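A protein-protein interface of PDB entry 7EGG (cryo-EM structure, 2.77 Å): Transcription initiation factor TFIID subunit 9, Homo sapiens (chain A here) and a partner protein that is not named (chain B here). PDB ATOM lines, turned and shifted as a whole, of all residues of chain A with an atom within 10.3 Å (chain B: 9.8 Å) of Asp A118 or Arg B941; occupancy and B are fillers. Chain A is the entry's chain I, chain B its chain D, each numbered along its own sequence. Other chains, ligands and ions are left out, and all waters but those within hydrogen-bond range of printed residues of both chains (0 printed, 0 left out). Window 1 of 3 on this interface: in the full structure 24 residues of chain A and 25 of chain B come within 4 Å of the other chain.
Printed residues of chain A that touch a printed residue of chain B: Pro A113, Leu A115, Asp A118, Arg A119, Tyr A120, Thr A123, Ala A124, Pro A125, Asn A126 and Tyr A127.
Hydrophobic or aromatic side chains of chain A that line the printed part of chain B: Pro A113, Leu A115, Tyr A120, Pro A125 and Tyr A127.
Of the 15 printed residues of chain B, 9 touch a printed residue of chain A.
Printed residues of chain B that touch a printed residue of chain A: Lys B929, Gln B936, Ser B938, Asp B939, Val B940, Arg B941, Leu B944, Glu B948 and Arg B1061.
Hydrophobic or aromatic side chains of chain B that line the printed part of chain A: Val B940 and Leu B944.
Among the printed residues, Asp or Glu carboxylates within 4 Å of a Lys or Arg side-chain nitrogen of the other chain: Asp A118 with Arg B941 (3.6 Å).
NE2 of Gln B943 lies within hydrogen-bond range of O of Asp B939 (3.0 Å).
The guanidinium group (NH1) of Arg A119 sits at hydrogen-bond distance from the side-chain hydroxyl (OH) of Tyr A120 (2.5 Å).
Leu B944 touches Pro A113.
Glu B948 touches Pro A113.
CD1 of Leu A115 touches CD1 of Leu B944 (3.6 Å).
Arg B1061 touches Tyr A120 (CD to CE1, 3.6 Å).
Thr A123 touches Val B940 (CG2 to CG1, 3.9 Å).
Thr A123 touches Leu B944.
Gln B936 touches Pro A125 (CG to O, 3.3 Å).
Pro A125 touches Asp B939.
Lys B929 touches Tyr A127.
NE of Arg B941 is in salt-bridge range of OD2 of Asp A118.
The backbone carbonyl oxygen of Thr A123 sits at hydrogen-bond distance from the guanidinium group of Arg B941 (2.7 Å).
The backbone carbonyl oxygen (O) of Ala A124 sits close to the backbone carbonyl oxygen (O) of Ser B938 (3.1 Å).
The guanidinium group (NH1) of Arg B1061 sits at hydrogen-bond distance from the backbone carbonyl oxygen (O) of Arg A119.
OH of Tyr A127 sits close to OE1 of Gln B936.
N of Ser B938 lies close to O of Pro A125 (3.5 Å).
The side-chain hydroxyl (OG) of Ser B938 is in hydrogen-bond range of the side-chain amide nitrogen (ND2) of Asn A126.
Asp A118 touches just one residue of chain B: Arg B941.
No residue of chain B comes within 4 Å of Pro A117.
Cys A121 touches none of the printed residues of chain B.
Printed residues of chain B within 4 Å of Thr A123: Val B940, Arg B941 and Leu B944.
Of chain B, only Ser B938 (3.1 Å) comes within 4 Å of Ala A124.
Of chain A, only Pro A125 (3.8 Å) comes within 4 Å of Asp B939.
No residue of chain A comes within 4 Å of Ala B942.
Of chain A, only Pro A113 (3.6 Å), Leu A115 (3.6 Å) and Thr A123 (3.9 Å) come within 4 Å of Leu B944.
Of the printed residues of chain A, Gln B936 touches Pro A125 (3.3 Å) and Tyr A127 (3.4 Å).
Of the printed residues of chain B, Pro A113 touches Leu B944 (3.6 Å) and Glu B948 (3.8 Å).
Of the printed residues of chain B, Leu A115 touches Leu B944.
Printed residues of chain A within 4 Å of Lys B929: Tyr A127.
Of the printed residues of chain B, Tyr A120 touches Arg B1061 (3.6 Å).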
ATOM      1  N   SER A 111      27.986  43.026 -22.965  1.00  0.00           N
ATOM      2  CA  SER A 111      28.306  41.732 -22.373  1.00  0.00           C
ATOM      3  C   SER A 111      27.206  40.708 -22.612  1.00  0.00           C
ATOM      4  O   SER A 111      27.473  39.501 -22.602  1.00  0.00           O
ATOM      5  CB  SER A 111      28.560  41.896 -20.876  1.00  0.00           C
ATOM      6  OG  SER A 111      27.579  42.731 -20.288  1.00  0.00           O
ATOM      7  N   PRO A 113      23.241  39.163 -21.653  1.00  0.00           N
ATOM      8  CA  PRO A 113      22.411  39.077 -20.445  1.00  0.00           C
ATOM      9  C   PRO A 113      23.260  39.167 -19.189  1.00  0.00           C
ATOM     10  O   PRO A 113      24.049  38.264 -18.899  1.00  0.00           O
ATOM     11  CB  PRO A 113      21.732  37.707 -20.577  1.00  0.00           C
ATOM     12  CG  PRO A 113      22.568  36.948 -21.543  1.00  0.00           C
ATOM     13  CD  PRO A 113      23.143  37.952 -22.481  1.00  0.00           C
ATOM     14  N   ARG A 114      23.115  40.261 -18.444  1.00  0.00           N
ATOM     15  CA  ARG A 114      23.966  40.526 -17.289  1.00  0.00           C
ATOM     16  C   ARG A 114      23.564  39.619 -16.137  1.00  0.00           C
ATOM     17  O   ARG A 114      22.492  39.787 -15.548  1.00  0.00           O
ATOM     18  CB  ARG A 114      23.865  41.993 -16.890  1.00  0.00           C
ATOM     19  CG  ARG A 114      24.736  42.916 -17.713  1.00  0.00           C
ATOM     20  CD  ARG A 114      24.036  44.233 -17.949  1.00  0.00           C
ATOM     21  NE  ARG A 114      24.722  45.051 -18.940  1.00  0.00           N
ATOM     22  CZ  ARG A 114      24.135  46.018 -19.633  1.00  0.00           C
ATOM     23  NH1 ARG A 114      22.852  46.287 -19.437  1.00  0.00           N
ATOM     24  NH2 ARG A 114      24.830  46.717 -20.521  1.00  0.00           N
ATOM     25  N   LEU A 115      24.429  38.671 -15.805  1.00  0.00           N
ATOM     26  CA  LEU A 115      24.165  37.650 -14.805  1.00  0.00           C
ATOM     27  C   LEU A 115      25.406  37.470 -13.945  1.00  0.00           C
ATOM     28  O   LEU A 115      26.507  37.856 -14.349  1.00  0.00           O
ATOM     29  CB  LEU A 115      23.779  36.319 -15.463  1.00  0.00           C
ATOM     30  CG  LEU A 115      22.342  36.141 -15.951  1.00  0.00           C
ATOM     31  CD1 LEU A 115      22.072  34.674 -16.147  1.00  0.00           C
ATOM     32  CD2 LEU A 115      21.342  36.733 -14.982  1.00  0.00           C
ATOM     33  N   PRO A 116      25.259  36.884 -12.755  1.00  0.00           N
ATOM     34  CA  PRO A 116      26.427  36.479 -11.957  1.00  0.00           C
ATOM     35  C   PRO A 116      27.214  35.363 -12.626  1.00  0.00           C
ATOM     36  O   PRO A 116      26.815  34.861 -13.688  1.00  0.00           O
ATOM     37  CB  PRO A 116      25.784  36.000 -10.645  1.00  0.00           C
ATOM     38  CG  PRO A 116      24.574  36.799 -10.525  1.00  0.00           C
ATOM     39  CD  PRO A 116      24.051  36.960 -11.917  1.00  0.00           C
ATOM     40  N   PRO A 117      28.364  34.969 -12.059  1.00  0.00           N
ATOM     41  CA  PRO A 117      29.024  33.739 -12.514  1.00  0.00           C
ATOM     42  C   PRO A 117      28.116  32.521 -12.399  1.00  0.00           C
ATOM     43  O   PRO A 117      27.225  32.460 -11.551  1.00  0.00           O
ATOM     44  CB  PRO A 117      30.229  33.624 -11.580  1.00  0.00           C
ATOM     45  CG  PRO A 117      30.581  35.026 -11.295  1.00  0.00           C
ATOM     46  CD  PRO A 117      29.294  35.806 -11.273  1.00  0.00           C
ATOM     47  N   ASP A 118      28.362  31.546 -13.280  1.00  0.00           N
ATOM     48  CA  ASP A 118      27.408  30.469 -13.528  1.00  0.00           C
ATOM     49  C   ASP A 118      27.248  29.517 -12.351  1.00  0.00           C
ATOM     50  O   ASP A 118      26.271  28.761 -12.316  1.00  0.00           O
ATOM     51  CB  ASP A 118      27.823  29.685 -14.772  1.00  0.00           C
ATOM     52  CG  ASP A 118      27.930  30.560 -16.003  1.00  0.00           C
ATOM     53  OD1 ASP A 118      27.652  31.772 -15.897  1.00  0.00           O
ATOM     54  OD2 ASP A 118      28.292  30.037 -17.075  1.00  0.00           O
ATOM     55  N   ARG A 119      28.170  29.528 -11.393  1.00  0.00           N
ATOM     56  CA  ARG A 119      27.989  28.772 -10.163  1.00  0.00           C
ATOM     57  C   ARG A 119      27.141  29.510  -9.138  1.00  0.00           C
ATOM     58  O   ARG A 119      26.879  28.959  -8.064  1.00  0.00           O
ATOM     59  CB  ARG A 119      29.346  28.418  -9.560  1.00  0.00           C
ATOM     60  CG  ARG A 119      30.249  29.607  -9.325  1.00  0.00           C
ATOM     61  CD  ARG A 119      31.629  29.151  -8.900  1.00  0.00           C
ATOM     62  NE  ARG A 119      32.252  30.084  -7.968  1.00  0.00           N
ATOM     63  CZ  ARG A 119      32.083  30.044  -6.651  1.00  0.00           C
ATOM     64  NH1 ARG A 119      32.690  30.932  -5.876  1.00  0.00           N
ATOM     65  NH2 ARG A 119      31.305  29.117  -6.109  1.00  0.00           N
ATOM     66  N   TYR A 120      26.710  30.732  -9.436  1.00  0.00           N
ATOM     67  CA  TYR A 120      25.807  31.482  -8.578  1.00  0.00           C
ATOM     68  C   TYR A 120      24.427  31.654  -9.191  1.00  0.00           C
ATOM     69  O   TYR A 120      23.529  32.183  -8.529  1.00  0.00           O
ATOM     70  CB  TYR A 120      26.402  32.857  -8.257  1.00  0.00           C
ATOM     71  CG  TYR A 120      27.645  32.790  -7.402  1.00  0.00           C
ATOM     72  CD1 TYR A 120      27.554  32.594  -6.031  1.00  0.00           C
ATOM     73  CD2 TYR A 120      28.906  32.919  -7.965  1.00  0.00           C
ATOM     74  CE1 TYR A 120      28.684  32.533  -5.246  1.00  0.00           C
ATOM     75  CE2 TYR A 120      30.042  32.855  -7.188  1.00  0.00           C
ATOM     76  CZ  TYR A 120      29.924  32.661  -5.829  1.00  0.00           C
ATOM     77  OH  TYR A 120      31.050  32.599  -5.044  1.00  0.00           O
ATOM     78  N   CYS A 121      24.237  31.222 -10.434  1.00  0.00           N
ATOM     79  CA  CYS A 121      22.955  31.289 -11.110  1.00  0.00           C
ATOM     80  C   CYS A 121      22.269  29.928 -11.061  1.00  0.00           C
ATOM     81  O   CYS A 121      22.803  28.951 -10.535  1.00  0.00           O
ATOM     82  CB  CYS A 121      23.137  31.758 -12.553  1.00  0.00           C
ATOM     83  SG  CYS A 121      24.032  33.303 -12.726  1.00  0.00           S
ATOM     84  N   LEU A 122      21.064  29.868 -11.618  1.00  0.00           N
ATOM     85  CA  LEU A 122      20.280  28.644 -11.705  1.00  0.00           C
ATOM     86  C   LEU A 122      20.107  28.211 -13.156  1.00  0.00           C
ATOM     87  O   LEU A 122      19.023  27.814 -13.578  1.00  0.00           O
ATOM     88  CB  LEU A 122      18.919  28.819 -11.039  1.00  0.00           C
ATOM     89  CG  LEU A 122      18.917  29.332  -9.605  1.00  0.00           C
ATOM     90  CD1 LEU A 122      17.500  29.539  -9.130  1.00  0.00           C
ATOM     91  CD2 LEU A 122      19.648  28.371  -8.699  1.00  0.00           C
ATOM     92  N   THR A 123      21.176  28.301 -13.939  1.00  0.00           N
ATOM     93  CA  THR A 123      21.147  27.997 -15.367  1.00  0.00           C
ATOM     94  C   THR A 123      22.137  26.870 -15.647  1.00  0.00           C
ATOM     95  O   THR A 123      23.302  27.121 -15.952  1.00  0.00           O
ATOM     96  CB  THR A 123      21.472  29.234 -16.182  1.00  0.00           C
ATOM     97  OG1 THR A 123      22.694  29.810 -15.707  1.00  0.00           O
ATOM     98  CG2 THR A 123      20.366  30.256 -16.055  1.00  0.00           C
ATOM     99  N   ALA A 124      21.667  25.636 -15.550  1.00  0.00           N
ATOM    100  CA  ALA A 124      22.434  24.428 -15.798  1.00  0.00           C
ATOM    101  C   ALA A 124      21.650  23.574 -16.784  1.00  0.00           C
ATOM    102  O   ALA A 124      20.464  23.835 -17.015  1.00  0.00           O
ATOM    103  CB  ALA A 124      22.684  23.671 -14.484  1.00  0.00           C
ATOM    104  N   PRO A 125      22.287  22.575 -17.422  1.00  0.00           N
ATOM    105  CA  PRO A 125      21.557  21.746 -18.405  1.00  0.00           C
ATOM    106  C   PRO A 125      20.357  20.970 -17.871  1.00  0.00           C
ATOM    107  O   PRO A 125      19.524  20.559 -18.688  1.00  0.00           O
ATOM    108  CB  PRO A 125      22.642  20.796 -18.914  1.00  0.00           C
ATOM    109  CG  PRO A 125      23.851  21.611 -18.884  1.00  0.00           C
ATOM    110  CD  PRO A 125      23.744  22.465 -17.651  1.00  0.00           C
ATOM    111  N   ASN A 126      20.250  20.756 -16.553  1.00  0.00           N
ATOM    112  CA  ASN A 126      19.001  20.430 -15.849  1.00  0.00           C
ATOM    113  C   ASN A 126      18.375  19.118 -16.344  1.00  0.00           C
ATOM    114  O   ASN A 126      17.310  19.094 -16.957  1.00  0.00           O
ATOM    115  CB  ASN A 126      18.010  21.592 -15.972  1.00  0.00           C
ATOM    116  CG  ASN A 126      16.955  21.559 -14.909  1.00  0.00           C
ATOM    117  OD1 ASN A 126      16.981  20.705 -14.030  1.00  0.00           O
ATOM    118  ND2 ASN A 126      16.015  22.491 -14.976  1.00  0.00           N
ATOM    119  N   TYR A 127      19.076  18.026 -16.062  1.00  0.00           N
ATOM    120  CA  TYR A 127      18.804  16.719 -16.647  1.00  0.00           C
ATOM    121  C   TYR A 127      17.561  16.062 -16.033  1.00  0.00           C
ATOM    122  O   TYR A 127      16.965  16.559 -15.076  1.00  0.00           O
ATOM    123  CB  TYR A 127      20.020  15.813 -16.476  1.00  0.00           C
ATOM    124  CG  TYR A 127      21.254  16.305 -17.198  1.00  0.00           C
ATOM    125  CD1 TYR A 127      22.120  17.219 -16.606  1.00  0.00           C
ATOM    126  CD2 TYR A 127      21.554  15.852 -18.474  1.00  0.00           C
ATOM    127  CE1 TYR A 127      23.244  17.663 -17.258  1.00  0.00           C
ATOM    128  CE2 TYR A 127      22.678  16.295 -19.137  1.00  0.00           C
ATOM    129  CZ  TYR A 127      23.518  17.200 -18.524  1.00  0.00           C
ATOM    130  OH  TYR A 127      24.640  17.645 -19.181  1.00  0.00           O
ATOM    131  N   LYS B 929      26.074  14.000 -17.600  1.00  0.00           N
ATOM    132  CA  LYS B 929      26.222  13.834 -19.042  1.00  0.00           C
ATOM    133  C   LYS B 929      27.124  12.669 -19.418  1.00  0.00           C
ATOM    134  O   LYS B 929      27.092  12.230 -20.572  1.00  0.00           O
ATOM    135  CB  LYS B 929      26.753  15.124 -19.666  1.00  0.00           C
ATOM    136  CG  LYS B 929      28.040  15.640 -19.052  1.00  0.00           C
ATOM    137  CD  LYS B 929      28.389  17.021 -19.587  1.00  0.00           C
ATOM    138  CE  LYS B 929      28.553  17.007 -21.098  1.00  0.00           C
ATOM    139  NZ  LYS B 929      28.954  18.341 -21.627  1.00  0.00           N
ATOM    140  N   GLN B 936      18.850  15.195 -21.084  1.00  0.00           N
ATOM    141  CA  GLN B 936      18.813  16.633 -20.874  1.00  0.00           C
ATOM    142  C   GLN B 936      17.411  17.167 -21.131  1.00  0.00           C
ATOM    143  O   GLN B 936      16.735  16.748 -22.075  1.00  0.00           O
ATOM    144  CB  GLN B 936      19.822  17.323 -21.789  1.00  0.00           C
ATOM    145  CG  GLN B 936      20.118  18.757 -21.417  1.00  0.00           C
ATOM    146  CD  GLN B 936      21.466  19.216 -21.917  1.00  0.00           C
ATOM    147  OE1 GLN B 936      22.482  18.570 -21.674  1.00  0.00           O
ATOM    148  NE2 GLN B 936      21.484  20.336 -22.623  1.00  0.00           N
ATOM    149  N   SER B 938      16.413  20.933 -20.144  1.00  0.00           N
ATOM    150  CA  SER B 938      16.346  22.371 -20.404  1.00  0.00           C
ATOM    151  C   SER B 938      17.718  22.978 -20.153  1.00  0.00           C
ATOM    152  O   SER B 938      18.138  23.090 -18.998  1.00  0.00           O
ATOM    153  CB  SER B 938      15.293  23.036 -19.527  1.00  0.00           C
ATOM    154  OG  SER B 938      15.677  23.000 -18.165  1.00  0.00           O
ATOM    155  N   ASP B 939      18.394  23.392 -21.221  1.00  0.00           N
ATOM    156  CA  ASP B 939      19.671  24.094 -21.124  1.00  0.00           C
ATOM    157  C   ASP B 939      19.402  25.584 -21.309  1.00  0.00           C
ATOM    158  O   ASP B 939      19.308  26.073 -22.436  1.00  0.00           O
ATOM    159  CB  ASP B 939      20.660  23.576 -22.160  1.00  0.00           C
ATOM    160  CG  ASP B 939      22.094  23.924 -21.823  1.00  0.00           C
ATOM    161  OD1 ASP B 939      22.321  24.575 -20.784  1.00  0.00           O
ATOM    162  OD2 ASP B 939      22.995  23.543 -22.598  1.00  0.00           O
ATOM    163  N   VAL B 940      19.457  26.387 -20.244  1.00  0.00           N
ATOM    164  CA  VAL B 940      19.142  27.841 -20.370  1.00  0.00           C
ATOM    165  C   VAL B 940      20.422  28.635 -20.565  1.00  0.00           C
ATOM    166  O   VAL B 940      20.370  29.690 -21.198  1.00  0.00           O
ATOM    167  CB  VAL B 940      18.283  28.403 -19.235  1.00  0.00           C
ATOM    168  CG1 VAL B 940      18.224  29.917 -19.285  1.00  0.00           C
ATOM    169  CG2 VAL B 940      16.882  27.824 -19.271  1.00  0.00           C
ATOM    170  N   ARG B 941      21.540  28.098 -20.116  1.00  0.00           N
ATOM    171  CA  ARG B 941      22.838  28.760 -20.295  1.00  0.00           C
ATOM    172  C   ARG B 941      23.087  28.901 -21.784  1.00  0.00           C
ATOM    173  O   ARG B 941      23.517  29.958 -22.173  1.00  0.00           O
ATOM    174  CB  ARG B 941      23.893  27.836 -19.706  1.00  0.00           C
ATOM    175  CG  ARG B 941      25.182  28.514 -19.280  1.00  0.00           C
ATOM    176  CD  ARG B 941      26.008  27.490 -18.531  1.00  0.00           C
ATOM    177  NE  ARG B 941      25.745  27.518 -17.102  1.00  0.00           N
ATOM    178  CZ  ARG B 941      26.135  26.582 -16.247  1.00  0.00           C
ATOM    179  NH1 ARG B 941      26.782  25.515 -16.681  1.00  0.00           N
ATOM    180  NH2 ARG B 941      25.849  26.706 -14.964  1.00  0.00           N
ATOM    181  N   ALA B 942      22.777  27.899 -22.589  1.00  0.00           N
ATOM    182  CA  ALA B 942      22.944  27.946 -24.055  1.00  0.00           C
ATOM    183  C   ALA B 942      22.059  28.993 -24.731  1.00  0.00           C
ATOM    184  O   ALA B 942      22.563  29.691 -25.649  1.00  0.00           O
ATOM    185  CB  ALA B 942      22.669  26.586 -24.568  1.00  0.00           C
ATOM    186  N   GLN B 943      20.810  29.137 -24.305  1.00  0.00           N
ATOM    187  CA  GLN B 943      19.911  30.191 -24.828  1.00  0.00           C
ATOM    188  C   GLN B 943      20.494  31.562 -24.465  1.00  0.00           C
ATOM    189  O   GLN B 943      20.496  32.516 -25.322  1.00  0.00           O
ATOM    190  CB  GLN B 943      18.567  29.928 -24.172  1.00  0.00           C
ATOM    191  CG  GLN B 943      18.031  28.531 -24.437  1.00  0.00           C
ATOM    192  CD  GLN B 943      16.682  28.290 -23.808  1.00  0.00           C
ATOM    193  OE1 GLN B 943      15.753  29.071 -23.961  1.00  0.00           O
ATOM    194  NE2 GLN B 943      16.559  27.185 -23.096  1.00  0.00           N
ATOM    195  N   LEU B 944      21.042  31.678 -23.260  1.00  0.00           N
ATOM    196  CA  LEU B 944      21.688  32.938 -22.833  1.00  0.00           C
ATOM    197  C   LEU B 944      22.926  33.216 -23.678  1.00  0.00           C
ATOM    198  O   LEU B 944      23.181  34.401 -23.987  1.00  0.00           O
ATOM    199  CB  LEU B 944      21.994  32.841 -21.343  1.00  0.00           C
ATOM    200  CG  LEU B 944      20.777  32.772 -20.428  1.00  0.00           C
ATOM    201  CD1 LEU B 944      21.217  32.685 -18.983  1.00  0.00           C
ATOM    202  CD2 LEU B 944      19.861  33.962 -20.645  1.00  0.00           C
ATOM    203  N   LYS B 945      23.677  32.189 -24.036  1.00  0.00           N
ATOM    204  CA  LYS B 945      24.858  32.351 -24.912  1.00  0.00           C
ATOM    205  C   LYS B 945      24.409  32.823 -26.283  1.00  0.00           C
ATOM    206  O   LYS B 945      25.085  33.702 -26.842  1.00  0.00           O
ATOM    207  CB  LYS B 945      25.715  31.090 -24.919  1.00  0.00           C
ATOM    208  CG  LYS B 945      27.103  31.238 -25.520  1.00  0.00           C
ATOM    209  CD  LYS B 945      27.143  30.943 -27.002  1.00  0.00           C
ATOM    210  CE  LYS B 945      26.630  29.560 -27.346  1.00  0.00           C
ATOM    211  NZ  LYS B 945      26.601  29.339 -28.810  1.00  0.00           N
ATOM    212  N   PHE B 946      23.292  32.319 -26.790  1.00  0.00           N
ATOM    213  CA  PHE B 946      22.761  32.849 -28.071  1.00  0.00           C
ATOM    214  C   PHE B 946      22.438  34.336 -27.935  1.00  0.00           C
ATOM    215  O   PHE B 946      22.816  35.134 -28.829  1.00  0.00           O
ATOM    216  CB  PHE B 946      21.426  32.201 -28.404  1.00  0.00           C
ATOM    217  CG  PHE B 946      20.877  32.527 -29.765  1.00  0.00           C
ATOM    218  CD1 PHE B 946      21.327  31.858 -30.888  1.00  0.00           C
ATOM    219  CD2 PHE B 946      19.896  33.488 -29.920  1.00  0.00           C
ATOM    220  CE1 PHE B 946      20.818  32.152 -32.139  1.00  0.00           C
ATOM    221  CE2 PHE B 946      19.390  33.783 -31.173  1.00  0.00           C
ATOM    222  CZ  PHE B 946      19.851  33.115 -32.279  1.00  0.00           C
ATOM    223  N   PHE B 947      21.817  34.731 -26.832  1.00  0.00           N
ATOM    224  CA  PHE B 947      21.556  36.179 -26.643  1.00  0.00           C
ATOM    225  C   PHE B 947      22.847  37.005 -26.595  1.00  0.00           C
ATOM    226  O   PHE B 947      22.905  38.101 -27.201  1.00  0.00           O
ATOM    227  CB  PHE B 947      20.619  36.394 -25.464  1.00  0.00           C
ATOM    228  CG  PHE B 947      19.271  35.752 -25.633  1.00  0.00           C
ATOM    229  CD1 PHE B 947      18.614  35.807 -26.847  1.00  0.00           C
ATOM    230  CD2 PHE B 947      18.660  35.098 -24.577  1.00  0.00           C
ATOM    231  CE1 PHE B 947      17.378  35.210 -27.008  1.00  0.00           C
ATOM    232  CE2 PHE B 947      17.422  34.501 -24.738  1.00  0.00           C
ATOM    233  CZ  PHE B 947      16.783  34.562 -25.953  1.00  0.00           C
ATOM    234  N   GLU B 948      23.883  36.503 -25.938  1.00  0.00           N
ATOM    235  CA  GLU B 948      25.192  37.209 -25.893  1.00  0.00           C
ATOM    236  C   GLU B 948      25.785  37.321 -27.289  1.00  0.00           C
ATOM    237  O   GLU B 948      26.362  38.361 -27.576  1.00  0.00           O
ATOM    238  CB  GLU B 948      26.162  36.521 -24.934  1.00  0.00           C
ATOM    239  CG  GLU B 948      27.352  35.853 -25.584  1.00  0.00           C
ATOM    240  CD  GLU B 948      28.064  34.880 -24.665  1.00  0.00           C
ATOM    241  OE1 GLU B 948      27.633  34.749 -23.502  1.00  0.00           O
ATOM    242  OE2 GLU B 948      29.043  34.249 -25.115  1.00  0.00           O
ATOM    243  N   GLN B 949      25.662  36.295 -28.120  1.00  0.00           N
ATOM    244  CA  GLN B 949      26.142  36.353 -29.520  1.00  0.00           C
ATOM    245  C   GLN B 949      25.379  37.408 -30.303  1.00  0.00           C
ATOM    246  O   GLN B 949      26.013  38.143 -31.063  1.00  0.00           O
ATOM    247  CB  GLN B 949      26.042  34.968 -30.139  1.00  0.00           C
ATOM    248  CG  GLN B 949      27.118  34.033 -29.616  1.00  0.00           C
ATOM    249  CD  GLN B 949      27.043  32.677 -30.263  1.00  0.00           C
ATOM    250  OE1 GLN B 949      25.996  32.264 -30.754  1.00  0.00           O
ATOM    251  NE2 GLN B 949      28.164  31.974 -30.267  1.00  0.00           N
ATOM    252  N   ARG B1061      29.748  28.624  -0.272  1.00  0.00           N
ATOM    253  CA  ARG B1061      28.346  28.283  -0.487  1.00  0.00           C
ATOM    254  C   ARG B1061      27.986  26.970   0.194  1.00  0.00           C
ATOM    255  O   ARG B1061      26.883  26.830   0.730  1.00  0.00           O
ATOM    256  CB  ARG B1061      28.039  28.185  -1.977  1.00  0.00           C
ATOM    257  CG  ARG B1061      28.744  29.187  -2.851  1.00  0.00           C
ATOM    258  CD  ARG B1061      28.200  29.100  -4.264  1.00  0.00           C
ATOM    259  NE  ARG B1061      26.798  29.503  -4.330  1.00  0.00           N
ATOM    260  CZ  ARG B1061      25.814  28.720  -4.758  1.00  0.00           C
ATOM    261  NH1 ARG B1061      26.076  27.486  -5.164  1.00  0.00           N
ATOM    262  NH2 ARG B1061      24.569  29.170  -4.783  1.00  0.00           N
